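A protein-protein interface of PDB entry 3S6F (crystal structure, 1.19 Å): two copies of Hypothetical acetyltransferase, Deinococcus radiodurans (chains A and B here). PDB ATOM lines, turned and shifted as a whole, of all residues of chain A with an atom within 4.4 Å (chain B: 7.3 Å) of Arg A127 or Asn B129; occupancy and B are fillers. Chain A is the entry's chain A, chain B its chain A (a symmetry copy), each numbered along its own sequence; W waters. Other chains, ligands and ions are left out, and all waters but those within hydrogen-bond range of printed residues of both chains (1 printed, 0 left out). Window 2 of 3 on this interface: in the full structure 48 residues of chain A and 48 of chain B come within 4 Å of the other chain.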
ATOM      1  N   LEU A 110     -16.632  26.341  16.290  1.00  0.00           N
ATOM      2  CA  LEU A 110     -15.175  26.248  16.295  1.00  0.00           C
ATOM      3  C   LEU A 110     -14.726  25.656  17.615  1.00  0.00           C
ATOM      4  O   LEU A 110     -15.479  25.636  18.577  1.00  0.00           O
ATOM      5  CB  LEU A 110     -14.512  27.614  16.015  1.00  0.00           C
ATOM      6  CG  LEU A 110     -14.791  28.705  17.052  1.00  0.00           C
ATOM      7  CD1 LEU A 110     -13.744  28.698  18.194  1.00  0.00           C
ATOM      8  CD2 LEU A 110     -14.821  30.066  16.358  1.00  0.00           C
ATOM      9  N   SER A 111     -13.504  25.158  17.620  1.00  0.00           N
ATOM     10  CA  SER A 111     -12.852  24.589  18.812  1.00  0.00           C
ATOM     11  C   SER A 111     -11.798  25.517  19.364  1.00  0.00           C
ATOM     12  O   SER A 111     -11.075  26.175  18.609  1.00  0.00           O
ATOM     13  CB  SER A 111     -12.201  23.245  18.505  1.00  0.00           C
ATOM     14  OG  SER A 111     -13.165  22.329  17.993  1.00  0.00           O
ATOM     15  N   CYS A 112     -11.656  25.551  20.688  1.00  0.00           N
ATOM     16  CA  CYS A 112     -10.566  26.330  21.260  1.00  0.00           C
ATOM     17  C   CYS A 112     -10.177  25.837  22.642  1.00  0.00           C
ATOM     18  O   CYS A 112     -10.920  25.117  23.302  1.00  0.00           O
ATOM     19  CB  CYS A 112     -10.908  27.820  21.271  1.00  0.00           C
ATOM     20  SG  CYS A 112     -12.115  28.308  22.510  1.00  0.00           S
ATOM     21  N   ASP A 113      -9.046  26.336  23.092  1.00  0.00           N
ATOM     22  CA  ASP A 113      -8.564  26.062  24.441  1.00  0.00           C
ATOM     23  C   ASP A 113      -9.171  27.047  25.439  1.00  0.00           C
ATOM     24  O   ASP A 113      -9.809  28.047  25.078  1.00  0.00           O
ATOM     25  CB  ASP A 113      -7.035  26.077  24.443  1.00  0.00           C
ATOM     26  CG  ASP A 113      -6.447  24.849  23.740  1.00  0.00           C
ATOM     27  OD1 ASP A 113      -6.930  23.727  24.012  1.00  0.00           O
ATOM     28  OD2 ASP A 113      -5.525  25.015  22.913  1.00  0.00           O
ATOM     29  N   ASP A 114      -8.996  26.755  26.721  1.00  0.00           N
ATOM     30  CA  ASP A 114      -9.607  27.607  27.728  1.00  0.00           C
ATOM     31  C   ASP A 114      -9.182  29.082  27.666  1.00  0.00           C
ATOM     32  O   ASP A 114      -9.995  29.976  27.861  1.00  0.00           O
ATOM     33  CB  ASP A 114      -9.263  27.085  29.136  1.00  0.00           C
ATOM     34  CG  ASP A 114     -10.007  25.792  29.502  1.00  0.00           C
ATOM     35  OD1 ASP A 114     -10.947  25.360  28.775  1.00  0.00           O
ATOM     36  OD2 ASP A 114      -9.660  25.188  30.544  1.00  0.00           O
ATOM     37  N   VAL A 117     -11.272  31.411  25.310  1.00  0.00           N
ATOM     38  CA  VAL A 117     -12.701  31.457  25.479  1.00  0.00           C
ATOM     39  C   VAL A 117     -13.250  32.894  25.589  1.00  0.00           C
ATOM     40  O   VAL A 117     -14.230  33.240  24.934  1.00  0.00           O
ATOM     41  CB  VAL A 117     -13.150  30.534  26.618  1.00  0.00           C
ATOM     42  CG1 VAL A 117     -14.604  30.836  26.984  1.00  0.00           C
ATOM     43  CG2 VAL A 117     -12.982  29.072  26.216  1.00  0.00           C
ATOM     44  N   GLU A 121     -16.285  34.710  23.550  1.00  0.00           N
ATOM     45  CA  GLU A 121     -17.500  35.126  24.251  1.00  0.00           C
ATOM     46  C   GLU A 121     -17.801  36.591  23.960  1.00  0.00           C
ATOM     47  O   GLU A 121     -18.975  36.973  23.777  1.00  0.00           O
ATOM     48  CB  GLU A 121     -17.394  34.876  25.747  1.00  0.00           C
ATOM     49  CG  GLU A 121     -17.486  33.374  26.036  1.00  0.00           C
ATOM     50  CD  GLU A 121     -17.393  32.983  27.492  1.00  0.00           C
ATOM     51  OE1 GLU A 121     -16.686  33.702  28.236  1.00  0.00           O
ATOM     52  OE2 GLU A 121     -17.979  31.918  27.851  1.00  0.00           O
ATOM     53  N   LYS A 126     -21.271  31.228  22.240  1.00  0.00           N
ATOM     54  CA  LYS A 126     -21.549  30.484  23.447  1.00  0.00           C
ATOM     55  C   LYS A 126     -20.694  29.248  23.517  1.00  0.00           C
ATOM     56  O   LYS A 126     -20.036  28.905  22.546  1.00  0.00           O
ATOM     57  CB  LYS A 126     -23.054  30.198  23.525  1.00  0.00           C
ATOM     58  CG  LYS A 126     -23.919  31.489  23.591  1.00  0.00           C
ATOM     59  CD  LYS A 126     -23.509  32.476  24.713  1.00  0.00           C
ATOM     60  CE  LYS A 126     -24.478  33.688  24.791  1.00  0.00           C
ATOM     61  NZ  LYS A 126     -23.814  35.013  25.114  1.00  0.00           N
ATOM     62  N   ARG A 127     -20.677  28.578  24.648  1.00  0.00           N
ATOM     63  CA  ARG A 127     -19.718  27.549  24.941  1.00  0.00           C
ATOM     64  C   ARG A 127     -20.382  26.186  25.138  1.00  0.00           C
ATOM     65  O   ARG A 127     -21.339  26.069  25.933  1.00  0.00           O
ATOM     66  CB  ARG A 127     -19.007  27.980  26.221  1.00  0.00           C
ATOM     67  CG  ARG A 127     -17.781  27.250  26.587  1.00  0.00           C
ATOM     68  CD  ARG A 127     -17.146  27.835  27.898  1.00  0.00           C
ATOM     69  NE  ARG A 127     -15.909  27.137  28.244  1.00  0.00           N
ATOM     70  CZ  ARG A 127     -15.097  27.481  29.240  1.00  0.00           C
ATOM     71  NH1 ARG A 127     -15.400  28.512  30.020  1.00  0.00           N
ATOM     72  NH2 ARG A 127     -13.995  26.781  29.461  1.00  0.00           N
ATOM     73  N   ALA A 128     -19.891  25.164  24.450  1.00  0.00           N
ATOM     74  CA  ALA A 128     -20.314  23.780  24.636  1.00  0.00           C
ATOM     75  C   ALA A 128     -19.058  22.902  24.587  1.00  0.00           C
ATOM     76  O   ALA A 128     -17.931  23.402  24.756  1.00  0.00           O
ATOM     77  CB  ALA A 128     -21.369  23.341  23.561  1.00  0.00           C
ATOM     78  N   ALA A 130     -16.319  20.702  22.561  1.00  0.00           N
ATOM     79  CA  ALA A 130     -15.709  20.339  21.255  1.00  0.00           C
ATOM     80  C   ALA A 130     -15.091  18.959  21.421  1.00  0.00           C
ATOM     81  O   ALA A 130     -14.191  18.777  22.251  1.00  0.00           O
ATOM     82  CB  ALA A 130     -14.650  21.342  20.832  1.00  0.00           C
ATOM     83  N   ASP B 109     -13.271  17.942  14.047  1.00  0.00           N
ATOM     84  CA  ASP B 109     -13.900  18.536  15.204  1.00  0.00           C
ATOM     85  C   ASP B 109     -15.418  18.506  15.090  1.00  0.00           C
ATOM     86  O   ASP B 109     -15.993  18.544  13.993  1.00  0.00           O
ATOM     87  CB  ASP B 109     -13.462  20.016  15.369  1.00  0.00           C
ATOM     88  CG  ASP B 109     -11.975  20.194  15.633  1.00  0.00           C
ATOM     89  OD1 ASP B 109     -11.149  19.890  14.730  1.00  0.00           O
ATOM     90  OD2 ASP B 109     -11.615  20.660  16.720  1.00  0.00           O
ATOM     91  N   LEU B 110     -16.094  18.493  16.237  1.00  0.00           N
ATOM     92  CA  LEU B 110     -17.549  18.584  16.306  1.00  0.00           C
ATOM     93  C   LEU B 110     -17.941  19.163  17.650  1.00  0.00           C
ATOM     94  O   LEU B 110     -17.147  19.172  18.579  1.00  0.00           O
ATOM     95  CB  LEU B 110     -18.224  17.222  16.040  1.00  0.00           C
ATOM     96  CG  LEU B 110     -17.901  16.120  17.053  1.00  0.00           C
ATOM     97  CD1 LEU B 110     -18.898  16.115  18.239  1.00  0.00           C
ATOM     98  CD2 LEU B 110     -17.901  14.766  16.344  1.00  0.00           C
ATOM     99  N   SER B 111     -19.161  19.660  17.713  1.00  0.00           N
ATOM    100  CA  SER B 111     -19.761  20.216  18.938  1.00  0.00           C
ATOM    101  C   SER B 111     -20.791  19.283  19.525  1.00  0.00           C
ATOM    102  O   SER B 111     -21.546  18.633  18.795  1.00  0.00           O
ATOM    103  CB  SER B 111     -20.425  21.564  18.673  1.00  0.00           C
ATOM    104  OG  SER B 111     -19.483  22.486  18.129  1.00  0.00           O
ATOM    105  N   CYS B 112     -20.876  19.235  20.853  1.00  0.00           N
ATOM    106  CA  CYS B 112     -21.941  18.449  21.464  1.00  0.00           C
ATOM    107  C   CYS B 112     -22.270  18.927  22.866  1.00  0.00           C
ATOM    108  O   CYS B 112     -21.498  19.641  23.501  1.00  0.00           O
ATOM    109  CB  CYS B 112     -21.598  16.960  21.444  1.00  0.00           C
ATOM    110  SG  CYS B 112     -20.339  16.459  22.625  1.00  0.00           S
ATOM    111  N   ASP B 113     -23.380  18.424  23.359  1.00  0.00           N
ATOM    112  CA  ASP B 113     -23.804  18.683  24.730  1.00  0.00           C
ATOM    113  C   ASP B 113     -23.155  17.689  25.691  1.00  0.00           C
ATOM    114  O   ASP B 113     -22.533  16.693  25.292  1.00  0.00           O
ATOM    115  CB  ASP B 113     -25.331  18.669  24.798  1.00  0.00           C
ATOM    116  CG  ASP B 113     -25.949  19.903  24.133  1.00  0.00           C
ATOM    117  OD1 ASP B 113     -25.454  21.023  24.397  1.00  0.00           O
ATOM    118  OD2 ASP B 113     -26.906  19.746  23.346  1.00  0.00           O
ATOM    119  N   ARG B 127     -11.693  16.168  24.389  1.00  0.00           N
ATOM    120  CA  ARG B 127     -12.639  17.194  24.734  1.00  0.00           C
ATOM    121  C   ARG B 127     -11.967  18.555  24.917  1.00  0.00           C
ATOM    122  O   ARG B 127     -10.977  18.664  25.671  1.00  0.00           O
ATOM    123  CB  ARG B 127     -13.294  16.750  26.039  1.00  0.00           C
ATOM    124  CG  ARG B 127     -14.504  17.476  26.465  1.00  0.00           C
ATOM    125  CD  ARG B 127     -15.081  16.877  27.796  1.00  0.00           C
ATOM    126  NE  ARG B 127     -16.302  17.570  28.203  1.00  0.00           N
ATOM    127  CZ  ARG B 127     -17.071  17.216  29.229  1.00  0.00           C
ATOM    128  NH1 ARG B 127     -16.735  16.177  29.984  1.00  0.00           N
ATOM    129  NH2 ARG B 127     -18.163  17.914  29.504  1.00  0.00           N
ATOM    130  N   ALA B 128     -12.487  19.584  24.261  1.00  0.00           N
ATOM    131  CA  ALA B 128     -12.056  20.966  24.443  1.00  0.00           C
ATOM    132  C   ALA B 128     -13.313  21.845  24.458  1.00  0.00           C
ATOM    133  O   ALA B 128     -14.431  21.343  24.670  1.00  0.00           O
ATOM    134  CB  ALA B 128     -11.048  21.416  23.329  1.00  0.00           C
ATOM    135  N   ASN B 129     -13.171  23.147  24.201  1.00  0.00           N
ATOM    136  CA  ASN B 129     -14.316  24.045  24.181  1.00  0.00           C
ATOM    137  C   ASN B 129     -14.834  24.196  22.761  1.00  0.00           C
ATOM    138  O   ASN B 129     -14.047  24.500  21.861  1.00  0.00           O
ATOM    139  CB  ASN B 129     -13.933  25.420  24.694  1.00  0.00           C
ATOM    140  CG  ASN B 129     -13.323  25.378  26.074  1.00  0.00           C
ATOM    141  OD1 ASN B 129     -14.034  25.161  27.043  1.00  0.00           O
ATOM    142  ND2 ASN B 129     -12.026  25.530  26.160  1.00  0.00           N
ATOM    143  N   ALA B 130     -16.136  24.065  22.575  1.00  0.00           N
ATOM    144  CA  ALA B 130     -16.801  24.441  21.300  1.00  0.00           C
ATOM    145  C   ALA B 130     -17.411  25.819  21.507  1.00  0.00           C
ATOM    146  O   ALA B 130     -18.275  25.993  22.377  1.00  0.00           O
ATOM    147  CB  ALA B 130     -17.878  23.443  20.913  1.00  0.00           C
ATOM    148  N   MET B 131     -16.968  26.794  20.732  1.00  0.00           N
ATOM    149  CA  MET B 131     -17.605  28.103  20.733  1.00  0.00           C
ATOM    150  C   MET B 131     -18.525  28.129  19.521  1.00  0.00           C
ATOM    151  O   MET B 131     -18.147  27.695  18.427  1.00  0.00           O
ATOM    152  CB  MET B 131     -16.576  29.211  20.619  1.00  0.00           C
ATOM    153  CG  MET B 131     -15.461  29.129  21.655  1.00  0.00           C
ATOM    154  SD  MET B 131     -16.073  29.079  23.511  1.00  0.00           S
ATOM    155  CE  MET B 131     -17.195  30.692  23.519  1.00  0.00           C
ATOM    156  N   PHE B 132     -19.742  28.577  19.710  1.00  0.00           N
ATOM    157  CA  PHE B 132     -20.755  28.454  18.680  1.00  0.00           C
ATOM    158  C   PHE B 132     -21.771  29.562  18.647  1.00  0.00           C
ATOM    159  O   PHE B 132     -22.000  30.277  19.617  1.00  0.00           O
ATOM    160  CB  PHE B 132     -21.446  27.077  18.778  1.00  0.00           C
ATOM    161  CG  PHE B 132     -22.389  26.969  19.948  1.00  0.00           C
ATOM    162  CD1 PHE B 132     -21.918  26.598  21.198  1.00  0.00           C
ATOM    163  CD2 PHE B 132     -23.733  27.281  19.824  1.00  0.00           C
ATOM    164  CE1 PHE B 132     -22.773  26.545  22.306  1.00  0.00           C
ATOM    165  CE2 PHE B 132     -24.597  27.212  20.907  1.00  0.00           C
ATOM    166  CZ  PHE B 132     -24.104  26.859  22.148  1.00  0.00           C
HETATM  167  O   HOH W   1     -16.591  23.781  27.487  1.00  0.00           O
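Of the 11 printed residues of chain A, 11 touch a printed residue of chain B. Of the 11 printed residues of chain B, 9 touch a printed residue of chain A. Hydrophobic or aromatic side chains of chain B within 4 Å of the printed part of chain A: Ala B128, Ala B130, Met B131 and Phe B132. Among the printed residues, no Asp or Glu carboxylate lies within 4 Å of a Lys or Arg side-chain nitrogen of the other chain.
OD1 of Asp A114 is in salt-bridge range of NH2 of Arg A127.
Of the printed residues of chain A, Asn B129 touches Leu A110 (3.8 Å), Ser A111 (3.3 Å), Cys A112 (2.9 Å), Asp A113 (3.3 Å), Asp A114 (2.8 Å), Val A117 (3.7 Å), Arg A127 (2.9 Å), Ala A128 (3.7 Å) and Ala A130 (3.4 Å). Printed residues of chain A within 4 Å of Met B131: Leu A110, Cys A112, Glu A121, Lys A126 and Arg A127. Printed residues of chain A within 4 Å of Leu B110: Ala A130 (3.3 Å). Printed residues of chain A within 4 Å of Ala B128: Cys A112 (3.7 Å) and Ala A130 (2.8 Å). Asp B113 touches none of the printed residues of chain A. Ser B111 touches none of the printed residues of chain A. The nearest printed residue of chain B that does not touch Arg A127 is Asp B113 (6.7 Å). The nearest printed residue of chain A that does not touch Ala B128 is Ala A128 (4.1 Å).
OG of Ser A111 sits at hydrogen-bond distance from OD2 of Asp B109 (2.6 Å). O of Lys A126 lies within hydrogen-bond range of N of Phe B132 (2.9 Å). The backbone NH (N) of Met B131 lies within hydrogen-bond range of the backbone carbonyl oxygen (O) of Leu A110 (2.9 Å). The backbone NH (N) of Ala A128 sits at hydrogen-bond distance from the backbone carbonyl oxygen (O) of Ala B130 (2.8 Å). The backbone NH (N) of Ala B128 is in hydrogen-bond range of the backbone carbonyl oxygen (O) of Ala A130, at 2.8 Å. The side-chain carboxylate (OD1) of Asp A114 lies within hydrogen-bond range of the side-chain amide nitrogen (ND2) of Asn B129 (2.8 Å). The side-chain amide oxygen of Asn B129 sits at hydrogen-bond distance from the guanidinium group of Arg A127 (2.9 Å). The backbone carbonyl oxygen of Ala B130 lies close to the backbone carbonyl oxygen of Lys A126 (3.4 Å). The backbone NH (N) of Cys A112 lies within hydrogen-bond range of the backbone carbonyl oxygen (O) of Asn B129, 2.9 Å away. The backbone NH (N) of Ala A130 lies close to the backbone NH (N) of Ala B130 (3.4 Å).
Among the printed residues, pairs that only touch across the chains: Leu A110 with Asn B129, Leu A110 with Ala B130, Ser A111 with Asn B129, Cys A112 with Ala B128, Cys A112 with Met B131, Asp A113 with Asn B129, Val A117 with Asn B129, Glu A121 with Met B131, Lys A126 with Met B131, Arg A127 with Ala B130, Arg A127 with Met B131, Arg A127 with Phe B132, Ala A128 with Cys B112, Ala A128 with Asn B129, Ala A128 with Phe B132, Ala A130 with Leu B110, Ala A130 with Arg B127 and Ala A130 with Asn B129.
Cys A112 touches Ala B128, and with the chains exchanged Ala A128 touches Cys B112. Arg A127 touches Ala B130, and with the chains exchanged Ala A130 touches Arg B127. Ala A128 touches Ala B130, and with the chains exchanged Ala A130 touches Ala B128. Ala B130 touches its own counterpart, Ala A130. Positions printed for both chains: 110, 111, 112, 113, 127, 128 and 130.
Water W1 lies within hydrogen-bond range of the side-chain amide oxygen of Asn B129 (2.9 Å) and the backbone carbonyl oxygen of Ala A128 (3.1 Å).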
